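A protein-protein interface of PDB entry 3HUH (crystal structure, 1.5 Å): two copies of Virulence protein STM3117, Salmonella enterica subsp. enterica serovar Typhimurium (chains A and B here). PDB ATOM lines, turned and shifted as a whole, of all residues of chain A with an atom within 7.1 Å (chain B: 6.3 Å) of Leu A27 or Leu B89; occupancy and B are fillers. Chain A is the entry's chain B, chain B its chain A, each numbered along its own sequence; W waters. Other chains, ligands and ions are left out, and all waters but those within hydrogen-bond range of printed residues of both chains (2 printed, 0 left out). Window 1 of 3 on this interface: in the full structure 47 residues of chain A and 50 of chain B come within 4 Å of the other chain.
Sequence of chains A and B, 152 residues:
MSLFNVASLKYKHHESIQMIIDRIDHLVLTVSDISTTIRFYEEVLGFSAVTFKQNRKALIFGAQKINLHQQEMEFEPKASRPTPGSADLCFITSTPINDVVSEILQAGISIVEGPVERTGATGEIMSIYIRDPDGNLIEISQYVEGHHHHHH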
ATOM      1  N   ILE A  24      18.468 -19.897   1.651  1.00  0.00           N
ATOM      2  CA  ILE A  24      17.774 -18.888   0.864  1.00  0.00           C
ATOM      3  C   ILE A  24      18.760 -17.726   0.829  1.00  0.00           C
ATOM      4  O   ILE A  24      19.368 -17.400   1.849  1.00  0.00           O
ATOM      5  CB  ILE A  24      16.490 -18.401   1.567  1.00  0.00           C
ATOM      6  CG1 ILE A  24      15.477 -19.540   1.654  1.00  0.00           C
ATOM      7  CG2 ILE A  24      15.906 -17.206   0.820  1.00  0.00           C
ATOM      8  CD1 ILE A  24      14.301 -19.244   2.591  1.00  0.00           C
ATOM      9  N   ASP A  25      18.948 -17.121  -0.337  1.00  0.00           N
ATOM     10  CA  ASP A  25      19.856 -15.990  -0.447  1.00  0.00           C
ATOM     11  C   ASP A  25      19.045 -14.716  -0.342  1.00  0.00           C
ATOM     12  O   ASP A  25      19.398 -13.784   0.382  1.00  0.00           O
ATOM     13  CB  ASP A  25      20.577 -15.998  -1.791  1.00  0.00           C
ATOM     14  CG  ASP A  25      21.603 -14.890  -1.894  1.00  0.00           C
ATOM     15  OD1 ASP A  25      22.676 -15.028  -1.278  1.00  0.00           O
ATOM     16  OD2 ASP A  25      21.332 -13.873  -2.573  1.00  0.00           O
ATOM     17  N   HIS A  26      17.943 -14.682  -1.077  1.00  0.00           N
ATOM     18  CA  HIS A  26      17.082 -13.514  -1.087  1.00  0.00           C
ATOM     19  C   HIS A  26      15.720 -13.885  -1.639  1.00  0.00           C
ATOM     20  O   HIS A  26      15.483 -15.029  -2.023  1.00  0.00           O
ATOM     21  CB  HIS A  26      17.709 -12.419  -1.958  1.00  0.00           C
ATOM     22  CG  HIS A  26      17.924 -12.826  -3.385  1.00  0.00           C
ATOM     23  ND1 HIS A  26      16.942 -12.725  -4.349  1.00  0.00           N
ATOM     24  CD2 HIS A  26      19.014 -13.324  -4.014  1.00  0.00           C
ATOM     25  CE1 HIS A  26      17.420 -13.142  -5.509  1.00  0.00           C
ATOM     26  NE2 HIS A  26      18.676 -13.510  -5.333  1.00  0.00           N
ATOM     27  N   LEU A  27      14.825 -12.905  -1.657  1.00  0.00           N
ATOM     28  CA  LEU A  27      13.484 -13.083  -2.193  1.00  0.00           C
ATOM     29  C   LEU A  27      13.003 -11.707  -2.602  1.00  0.00           C
ATOM     30  O   LEU A  27      13.589 -10.697  -2.207  1.00  0.00           O
ATOM     31  CB  LEU A  27      12.558 -13.710  -1.147  1.00  0.00           C
ATOM     32  CG  LEU A  27      12.362 -12.996   0.185  1.00  0.00           C
ATOM     33  CD1 LEU A  27      11.268 -11.938   0.074  1.00  0.00           C
ATOM     34  CD2 LEU A  27      11.978 -14.032   1.232  1.00  0.00           C
ATOM     35  N   VAL A  28      11.946 -11.661  -3.403  1.00  0.00           N
ATOM     36  CA  VAL A  28      11.425 -10.388  -3.873  1.00  0.00           C
ATOM     37  C   VAL A  28      10.053 -10.061  -3.324  1.00  0.00           C
ATOM     38  O   VAL A  28       9.138 -10.886  -3.375  1.00  0.00           O
ATOM     39  CB  VAL A  28      11.322 -10.366  -5.413  1.00  0.00           C
ATOM     40  CG1 VAL A  28      10.804  -9.014  -5.879  1.00  0.00           C
ATOM     41  CG2 VAL A  28      12.677 -10.675  -6.035  1.00  0.00           C
ATOM     42  N   LEU A  29       9.918  -8.854  -2.787  1.00  0.00           N
ATOM     43  CA  LEU A  29       8.637  -8.395  -2.287  1.00  0.00           C
ATOM     44  C   LEU A  29       8.118  -7.370  -3.283  1.00  0.00           C
ATOM     45  O   LEU A  29       8.862  -6.483  -3.705  1.00  0.00           O
ATOM     46  CB  LEU A  29       8.774  -7.724  -0.921  1.00  0.00           C
ATOM     47  CG  LEU A  29       8.999  -8.603   0.310  1.00  0.00           C
ATOM     48  CD1 LEU A  29       8.989  -7.724   1.547  1.00  0.00           C
ATOM     49  CD2 LEU A  29       7.905  -9.667   0.410  1.00  0.00           C
ATOM     50  N   PHE A  61      20.310  -7.668   5.627  1.00  0.00           N
ATOM     51  CA  PHE A  61      20.371  -8.092   7.022  1.00  0.00           C
ATOM     52  C   PHE A  61      21.146  -9.405   7.031  1.00  0.00           C
ATOM     53  O   PHE A  61      20.987 -10.225   6.127  1.00  0.00           O
ATOM     54  CB  PHE A  61      18.961  -8.300   7.580  1.00  0.00           C
ATOM     55  CG  PHE A  61      18.144  -9.287   6.802  1.00  0.00           C
ATOM     56  CD1 PHE A  61      18.144 -10.638   7.141  1.00  0.00           C
ATOM     57  CD2 PHE A  61      17.396  -8.871   5.705  1.00  0.00           C
ATOM     58  CE1 PHE A  61      17.411 -11.560   6.401  1.00  0.00           C
ATOM     59  CE2 PHE A  61      16.657  -9.786   4.954  1.00  0.00           C
ATOM     60  CZ  PHE A  61      16.663 -11.132   5.303  1.00  0.00           C
ATOM     61  N   LYS A  65      19.173 -10.853   1.837  1.00  0.00           N
ATOM     62  CA  LYS A  65      18.552  -9.587   1.464  1.00  0.00           C
ATOM     63  C   LYS A  65      17.167  -9.782   0.871  1.00  0.00           C
ATOM     64  O   LYS A  65      16.798 -10.884   0.470  1.00  0.00           O
ATOM     65  CB  LYS A  65      19.429  -8.817   0.467  1.00  0.00           C
ATOM     66  CG  LYS A  65      19.512  -9.427  -0.925  1.00  0.00           C
ATOM     67  CD  LYS A  65      20.082  -8.427  -1.930  1.00  0.00           C
ATOM     68  CE  LYS A  65      20.146  -9.016  -3.333  1.00  0.00           C
ATOM     69  NZ  LYS A  65      20.526  -7.997  -4.357  1.00  0.00           N
ATOM     70  N   ILE A  66      16.405  -8.698   0.838  1.00  0.00           N
ATOM     71  CA  ILE A  66      15.064  -8.705   0.279  1.00  0.00           C
ATOM     72  C   ILE A  66      15.043  -7.668  -0.833  1.00  0.00           C
ATOM     73  O   ILE A  66      15.252  -6.476  -0.581  1.00  0.00           O
ATOM     74  CB  ILE A  66      14.007  -8.295   1.333  1.00  0.00           C
ATOM     75  CG1 ILE A  66      13.990  -9.301   2.487  1.00  0.00           C
ATOM     76  CG2 ILE A  66      12.639  -8.154   0.672  1.00  0.00           C
ATOM     77  CD1 ILE A  66      13.620 -10.689   2.085  1.00  0.00           C
ATOM     78  N   ASN A  67      14.813  -8.109  -2.063  1.00  0.00           N
ATOM     79  CA  ASN A  67      14.747  -7.171  -3.178  1.00  0.00           C
ATOM     80  C   ASN A  67      13.341  -6.596  -3.240  1.00  0.00           C
ATOM     81  O   ASN A  67      12.361  -7.297  -2.974  1.00  0.00           O
ATOM     82  CB  ASN A  67      15.098  -7.861  -4.499  1.00  0.00           C
ATOM     83  CG  ASN A  67      16.569  -8.211  -4.600  1.00  0.00           C
ATOM     84  OD1 ASN A  67      17.425  -7.470  -4.112  1.00  0.00           O
ATOM     85  ND2 ASN A  67      16.873  -9.333  -5.243  1.00  0.00           N
ATOM     86  N   LEU A  68      13.235  -5.315  -3.582  1.00  0.00           N
ATOM     87  CA  LEU A  68      11.936  -4.667  -3.654  1.00  0.00           C
ATOM     88  C   LEU A  68      11.552  -4.272  -5.075  1.00  0.00           C
ATOM     89  O   LEU A  68      12.354  -3.691  -5.809  1.00  0.00           O
ATOM     90  CB  LEU A  68      11.922  -3.422  -2.759  1.00  0.00           C
ATOM     91  CG  LEU A  68      12.294  -3.622  -1.286  1.00  0.00           C
ATOM     92  CD1 LEU A  68      12.327  -2.282  -0.572  1.00  0.00           C
ATOM     93  CD2 LEU A  68      11.287  -4.557  -0.622  1.00  0.00           C
ATOM     94  N   ALA A  87       3.233 -12.014   1.266  1.00  0.00           N
ATOM     95  CA  ALA A  87       4.355 -12.656   1.933  1.00  0.00           C
ATOM     96  C   ALA A  87       4.041 -12.999   3.386  1.00  0.00           C
ATOM     97  O   ALA A  87       3.313 -12.278   4.067  1.00  0.00           O
ATOM     98  CB  ALA A  87       5.586 -11.761   1.859  1.00  0.00           C
ATOM     99  N   LEU A  89       6.605 -14.237   6.245  1.00  0.00           N
ATOM    100  CA  LEU A  89       8.010 -14.495   6.561  1.00  0.00           C
ATOM    101  C   LEU A  89       8.380 -14.533   8.030  1.00  0.00           C
ATOM    102  O   LEU A  89       7.780 -13.842   8.848  1.00  0.00           O
ATOM    103  CB  LEU A  89       8.882 -13.410   5.919  1.00  0.00           C
ATOM    104  CG  LEU A  89       8.565 -12.955   4.495  1.00  0.00           C
ATOM    105  CD1 LEU A  89       9.407 -11.731   4.153  1.00  0.00           C
ATOM    106  CD2 LEU A  89       8.839 -14.096   3.526  1.00  0.00           C
ATOM    107  N   PHE A  91      11.746 -14.141  10.634  1.00  0.00           N
ATOM    108  CA  PHE A  91      13.134 -13.737  10.826  1.00  0.00           C
ATOM    109  C   PHE A  91      13.563 -14.075  12.247  1.00  0.00           C
ATOM    110  O   PHE A  91      12.782 -13.919  13.189  1.00  0.00           O
ATOM    111  CB  PHE A  91      13.292 -12.220  10.651  1.00  0.00           C
ATOM    112  CG  PHE A  91      12.870 -11.711   9.309  1.00  0.00           C
ATOM    113  CD1 PHE A  91      13.678 -11.901   8.196  1.00  0.00           C
ATOM    114  CD2 PHE A  91      11.666 -11.033   9.159  1.00  0.00           C
ATOM    115  CE1 PHE A  91      13.293 -11.419   6.944  1.00  0.00           C
ATOM    116  CE2 PHE A  91      11.272 -10.548   7.915  1.00  0.00           C
ATOM    117  CZ  PHE A  91      12.088 -10.741   6.804  1.00  0.00           C
ATOM    118  N   ILE B  24      16.649 -15.402   7.863  1.00  0.00           N
ATOM    119  CA  ILE B  24      15.276 -15.835   7.619  1.00  0.00           C
ATOM    120  C   ILE B  24      15.250 -17.264   8.166  1.00  0.00           C
ATOM    121  O   ILE B  24      16.173 -18.040   7.909  1.00  0.00           O
ATOM    122  CB  ILE B  24      14.959 -15.865   6.107  1.00  0.00           C
ATOM    123  CG1 ILE B  24      14.819 -14.437   5.574  1.00  0.00           C
ATOM    124  CG2 ILE B  24      13.694 -16.684   5.848  1.00  0.00           C
ATOM    125  CD1 ILE B  24      14.823 -14.354   4.047  1.00  0.00           C
ATOM    126  N   LEU B  27       9.351 -19.466   5.836  1.00  0.00           N
ATOM    127  CA  LEU B  27       8.334 -18.655   5.200  1.00  0.00           C
ATOM    128  C   LEU B  27       7.211 -19.597   4.822  1.00  0.00           C
ATOM    129  O   LEU B  27       7.389 -20.816   4.803  1.00  0.00           O
ATOM    130  CB  LEU B  27       8.899 -17.933   3.969  1.00  0.00           C
ATOM    131  CG  LEU B  27       9.491 -18.760   2.831  1.00  0.00           C
ATOM    132  CD1 LEU B  27       8.398 -19.221   1.896  1.00  0.00           C
ATOM    133  CD2 LEU B  27      10.488 -17.908   2.074  1.00  0.00           C
ATOM    134  N   LEU B  29       4.309 -20.745   2.028  1.00  0.00           N
ATOM    135  CA  LEU B  29       3.835 -20.711   0.658  1.00  0.00           C
ATOM    136  C   LEU B  29       2.399 -21.211   0.684  1.00  0.00           C
ATOM    137  O   LEU B  29       2.107 -22.227   1.310  1.00  0.00           O
ATOM    138  CB  LEU B  29       4.664 -21.631  -0.249  1.00  0.00           C
ATOM    139  CG  LEU B  29       6.091 -21.208  -0.599  1.00  0.00           C
ATOM    140  CD1 LEU B  29       6.718 -22.253  -1.523  1.00  0.00           C
ATOM    141  CD2 LEU B  29       6.062 -19.841  -1.287  1.00  0.00           C
ATOM    142  N   TYR B  41       9.217 -30.002  -4.900  1.00  0.00           N
ATOM    143  CA  TYR B  41      10.361 -29.620  -4.081  1.00  0.00           C
ATOM    144  C   TYR B  41      11.243 -30.787  -3.658  1.00  0.00           C
ATOM    145  O   TYR B  41      12.461 -30.635  -3.535  1.00  0.00           O
ATOM    146  CB  TYR B  41       9.903 -28.790  -2.868  1.00  0.00           C
ATOM    147  CG  TYR B  41       9.536 -27.372  -3.262  1.00  0.00           C
ATOM    148  CD1 TYR B  41       8.236 -27.046  -3.644  1.00  0.00           C
ATOM    149  CD2 TYR B  41      10.510 -26.371  -3.329  1.00  0.00           C
ATOM    150  CE1 TYR B  41       7.909 -25.761  -4.087  1.00  0.00           C
ATOM    151  CE2 TYR B  41      10.196 -25.083  -3.777  1.00  0.00           C
ATOM    152  CZ  TYR B  41       8.898 -24.785  -4.156  1.00  0.00           C
ATOM    153  OH  TYR B  41       8.603 -23.522  -4.623  1.00  0.00           O
ATOM    154  N   ILE B  66      10.269 -24.329   4.626  1.00  0.00           N
ATOM    155  CA  ILE B  66       9.155 -23.650   3.990  1.00  0.00           C
ATOM    156  C   ILE B  66       7.893 -24.352   4.472  1.00  0.00           C
ATOM    157  O   ILE B  66       7.708 -25.546   4.232  1.00  0.00           O
ATOM    158  CB  ILE B  66       9.240 -23.738   2.454  1.00  0.00           C
ATOM    159  CG1 ILE B  66      10.382 -22.848   1.958  1.00  0.00           C
ATOM    160  CG2 ILE B  66       7.908 -23.321   1.827  1.00  0.00           C
ATOM    161  CD1 ILE B  66      10.653 -22.968   0.488  1.00  0.00           C
ATOM    162  N   ALA B  87       5.229 -15.996  -4.901  1.00  0.00           N
ATOM    163  CA  ALA B  87       6.585 -16.033  -4.368  1.00  0.00           C
ATOM    164  C   ALA B  87       7.658 -15.934  -5.447  1.00  0.00           C
ATOM    165  O   ALA B  87       7.487 -16.430  -6.565  1.00  0.00           O
ATOM    166  CB  ALA B  87       6.794 -17.301  -3.544  1.00  0.00           C
ATOM    167  N   ASP B  88       8.763 -15.297  -5.075  1.00  0.00           N
ATOM    168  CA  ASP B  88       9.923 -15.078  -5.939  1.00  0.00           C
ATOM    169  C   ASP B  88      11.085 -15.300  -4.971  1.00  0.00           C
ATOM    170  O   ASP B  88      11.452 -14.398  -4.217  1.00  0.00           O
ATOM    171  CB  ASP B  88       9.898 -13.633  -6.445  1.00  0.00           C
ATOM    172  CG  ASP B  88      10.948 -13.360  -7.493  1.00  0.00           C
ATOM    173  OD1 ASP B  88      11.992 -14.051  -7.494  1.00  0.00           O
ATOM    174  OD2 ASP B  88      10.732 -12.435  -8.304  1.00  0.00           O
ATOM    175  N   LEU B  89      11.644 -16.509  -4.996  1.00  0.00           N
ATOM    176  CA  LEU B  89      12.692 -16.921  -4.064  1.00  0.00           C
ATOM    177  C   LEU B  89      13.989 -17.372  -4.707  1.00  0.00           C
ATOM    178  O   LEU B  89      13.985 -17.992  -5.766  1.00  0.00           O
ATOM    179  CB  LEU B  89      12.176 -18.091  -3.220  1.00  0.00           C
ATOM    180  CG  LEU B  89      10.726 -18.056  -2.732  1.00  0.00           C
ATOM    181  CD1 LEU B  89      10.383 -19.381  -2.076  1.00  0.00           C
ATOM    182  CD2 LEU B  89      10.533 -16.902  -1.756  1.00  0.00           C
ATOM    183  N   CYS B  90      15.101 -17.091  -4.039  1.00  0.00           N
ATOM    184  CA  CYS B  90      16.404 -17.504  -4.537  1.00  0.00           C
ATOM    185  C   CYS B  90      17.066 -18.443  -3.539  1.00  0.00           C
ATOM    186  O   CYS B  90      17.199 -18.119  -2.357  1.00  0.00           O
ATOM    187  CB  CYS B  90      17.313 -16.298  -4.769  1.00  0.00           C
ATOM    188  SG  CYS B  90      18.999 -16.777  -5.242  1.00  0.00           S
ATOM    189  N   PHE B  91      17.477 -19.607  -4.028  1.00  0.00           N
ATOM    190  CA  PHE B  91      18.133 -20.613  -3.200  1.00  0.00           C
ATOM    191  C   PHE B  91      19.574 -20.779  -3.657  1.00  0.00           C
ATOM    192  O   PHE B  91      19.843 -20.826  -4.860  1.00  0.00           O
ATOM    193  CB  PHE B  91      17.418 -21.957  -3.342  1.00  0.00           C
ATOM    194  CG  PHE B  91      16.021 -21.963  -2.799  1.00  0.00           C
ATOM    195  CD1 PHE B  91      15.795 -22.007  -1.428  1.00  0.00           C
ATOM    196  CD2 PHE B  91      14.931 -21.907  -3.658  1.00  0.00           C
ATOM    197  CE1 PHE B  91      14.497 -21.995  -0.921  1.00  0.00           C
ATOM    198  CE2 PHE B  91      13.630 -21.893  -3.164  1.00  0.00           C
ATOM    199  CZ  PHE B  91      13.411 -21.937  -1.795  1.00  0.00           C
ATOM    200  N   ASN B 136       5.248 -19.962  -8.767  1.00  0.00           N
ATOM    201  CA  ASN B 136       6.223 -19.198  -8.002  1.00  0.00           C
ATOM    202  C   ASN B 136       7.531 -19.228  -8.786  1.00  0.00           C
ATOM    203  O   ASN B 136       7.866 -20.240  -9.417  1.00  0.00           O
ATOM    204  CB  ASN B 136       6.453 -19.824  -6.622  1.00  0.00           C
ATOM    205  CG  ASN B 136       5.211 -19.788  -5.744  1.00  0.00           C
ATOM    206  OD1 ASN B 136       4.836 -20.795  -5.141  1.00  0.00           O
ATOM    207  ND2 ASN B 136       4.578 -18.631  -5.660  1.00  0.00           N
ATOM    208  N   LEU B 137       8.262 -18.120  -8.765  1.00  0.00           N
ATOM    209  CA  LEU B 137       9.538 -18.065  -9.467  1.00  0.00           C
ATOM    210  C   LEU B 137      10.622 -18.565  -8.523  1.00  0.00           C
ATOM    211  O   LEU B 137      10.766 -18.061  -7.401  1.00  0.00           O
ATOM    212  CB  LEU B 137       9.851 -16.636  -9.910  1.00  0.00           C
ATOM    213  CG  LEU B 137      11.137 -16.475 -10.729  1.00  0.00           C
ATOM    214  CD1 LEU B 137      11.004 -17.203 -12.067  1.00  0.00           C
ATOM    215  CD2 LEU B 137      11.413 -15.001 -10.944  1.00  0.00           C
ATOM    216  N   ILE B 138      11.369 -19.565  -8.974  1.00  0.00           N
ATOM    217  CA  ILE B 138      12.441 -20.133  -8.171  1.00  0.00           C
ATOM    218  C   ILE B 138      13.771 -19.892  -8.870  1.00  0.00           C
ATOM    219  O   ILE B 138      13.997 -20.361  -9.983  1.00  0.00           O
ATOM    220  CB  ILE B 138      12.242 -21.647  -7.964  1.00  0.00           C
ATOM    221  CG1 ILE B 138      10.862 -21.914  -7.348  1.00  0.00           C
ATOM    222  CG2 ILE B 138      13.354 -22.198  -7.083  1.00  0.00           C
ATOM    223  CD1 ILE B 138      10.606 -21.204  -6.027  1.00  0.00           C
ATOM    224  N   GLU B 139      14.635 -19.140  -8.199  1.00  0.00           N
ATOM    225  CA  GLU B 139      15.953 -18.799  -8.707  1.00  0.00           C
ATOM    226  C   GLU B 139      16.950 -19.683  -7.964  1.00  0.00           C
ATOM    227  O   GLU B 139      17.063 -19.599  -6.744  1.00  0.00           O
ATOM    228  CB  GLU B 139      16.233 -17.312  -8.428  1.00  0.00           C
ATOM    229  CG  GLU B 139      17.553 -16.770  -8.981  1.00  0.00           C
ATOM    230  CD  GLU B 139      17.806 -15.311  -8.603  1.00  0.00           C
ATOM    231  OE1 GLU B 139      16.897 -14.668  -8.033  1.00  0.00           O
ATOM    232  OE2 GLU B 139      18.918 -14.798  -8.879  1.00  0.00           O
ATOM    233  N   ILE B 140      17.640 -20.556  -8.692  1.00  0.00           N
ATOM    234  CA  ILE B 140      18.640 -21.435  -8.082  1.00  0.00           C
ATOM    235  C   ILE B 140      19.991 -20.857  -8.487  1.00  0.00           C
ATOM    236  O   ILE B 140      20.289 -20.725  -9.680  1.00  0.00           O
ATOM    237  CB  ILE B 140      18.492 -22.885  -8.574  1.00  0.00           C
ATOM    238  CG1 ILE B 140      17.090 -23.397  -8.231  1.00  0.00           C
ATOM    239  CG2 ILE B 140      19.526 -23.768  -7.899  1.00  0.00           C
ATOM    240  CD1 ILE B 140      16.713 -24.699  -8.896  1.00  0.00           C
HETATM  241  O   HOH W   1       8.587 -13.516  -2.709  1.00  0.00           O
HETATM  242  O   HOH W   2      14.284 -14.098  -5.666  1.00  0.00           O
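The backbone carbonyl oxygen (O) of His A26 is in hydrogen-bond range of the backbone NH (N) of Cys B90 (2.9 Å). The backbone carbonyl oxygen (O) of Cys B90 is in hydrogen-bond range of the backbone NH (N) of Asp A25, 2.9 Å away. A ring nitrogen (NE2) of His A26 sits close to the side-chain carboxylate of Glu B139 (3.4 Å). The backbone carbonyl oxygen (O) of Asp B88 lies within hydrogen-bond range of the backbone NH (N) of Val A28 (2.9 Å).
N of Lys A65 sits at hydrogen-bond distance from O of Asp A25, at 3.3 Å. The side-chain sulfur of Cys B90 sits close to the backbone carbonyl oxygen of Glu B139 (3.7 Å). The backbone NH (N) of Leu B89 lies within hydrogen-bond range of the backbone carbonyl oxygen (O) of Leu B137, 3.0 Å away. O of Glu B139 is in hydrogen-bond range of N of Phe B91. N of Asn A67 sits at hydrogen-bond distance from O of Leu A27 (2.9 Å). O of Leu B89 lies within hydrogen-bond range of N of Glu B139.
Among the printed residues, merely in contact across the chains: Leu A27 with Asp B88 (3.2 Å), Ile A24 with Cys B90 (3.4 Å), Phe A91 with Ile B24 (3.6 Å), Ile A24 with Phe B91 (3.7 Å), Phe A61 with Ile B24 (3.8 Å), Leu A27 with Leu B89 (3.8 Å), Leu A89 with Leu B27 (3.9 Å) and His A26 with Leu B89 (3.9 Å).
Printed residues of chain B within 4 Å of Leu A27: Asp B88 and Leu B89. Printed residues of chain B within 4 Å of Phe A61: Ile B24. Printed residues of chain B within 4 Å of Phe A91: Ile B24 (3.6 Å). Of the printed residues of chain A, Phe B91 touches Ile A24 (3.7 Å). Printed residues of chain A within 4 Å of Glu B139: His A26 (3.0 Å).
Hydrophobic or aromatic side chains of chain B that line the printed part of chain A: Ile B24, Leu B27, Leu B89 and Phe B91. Of the 14 printed residues of chain A, 8 touch a printed residue of chain B. Hydrophobic or aromatic side chains of chain A that line the printed part of chain B: Ile A24, His A26, Leu A27, Val A28, Phe A61, Leu A89 and Phe A91. Among the printed residues, 12 pairs touch across the chains. Among the printed residues, no Asp or Glu carboxylate lies within 4 Å of a Lys or Arg side-chain nitrogen of the other chain.
Ile A24 touches Phe B91, and with the chains exchanged Phe A91 touches Ile B24. Leu A27 touches Leu B89, and with the chains exchanged Leu A89 touches Leu B27. Positions printed for both chains: 24, 27, 29, 66, 87, 89 and 91. Of the 12 pairs that touch across the chains among the printed residues, 4 have their exchanged pair printed and touching as well.
Water W1 bridges the backbone carbonyl oxygen (O) of Val A28 (2.8 Å) and the backbone NH (N) of Asp B88 (3.0 Å). Water W2 bridges OD1 of Asp B88 and ND1 of His A26.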
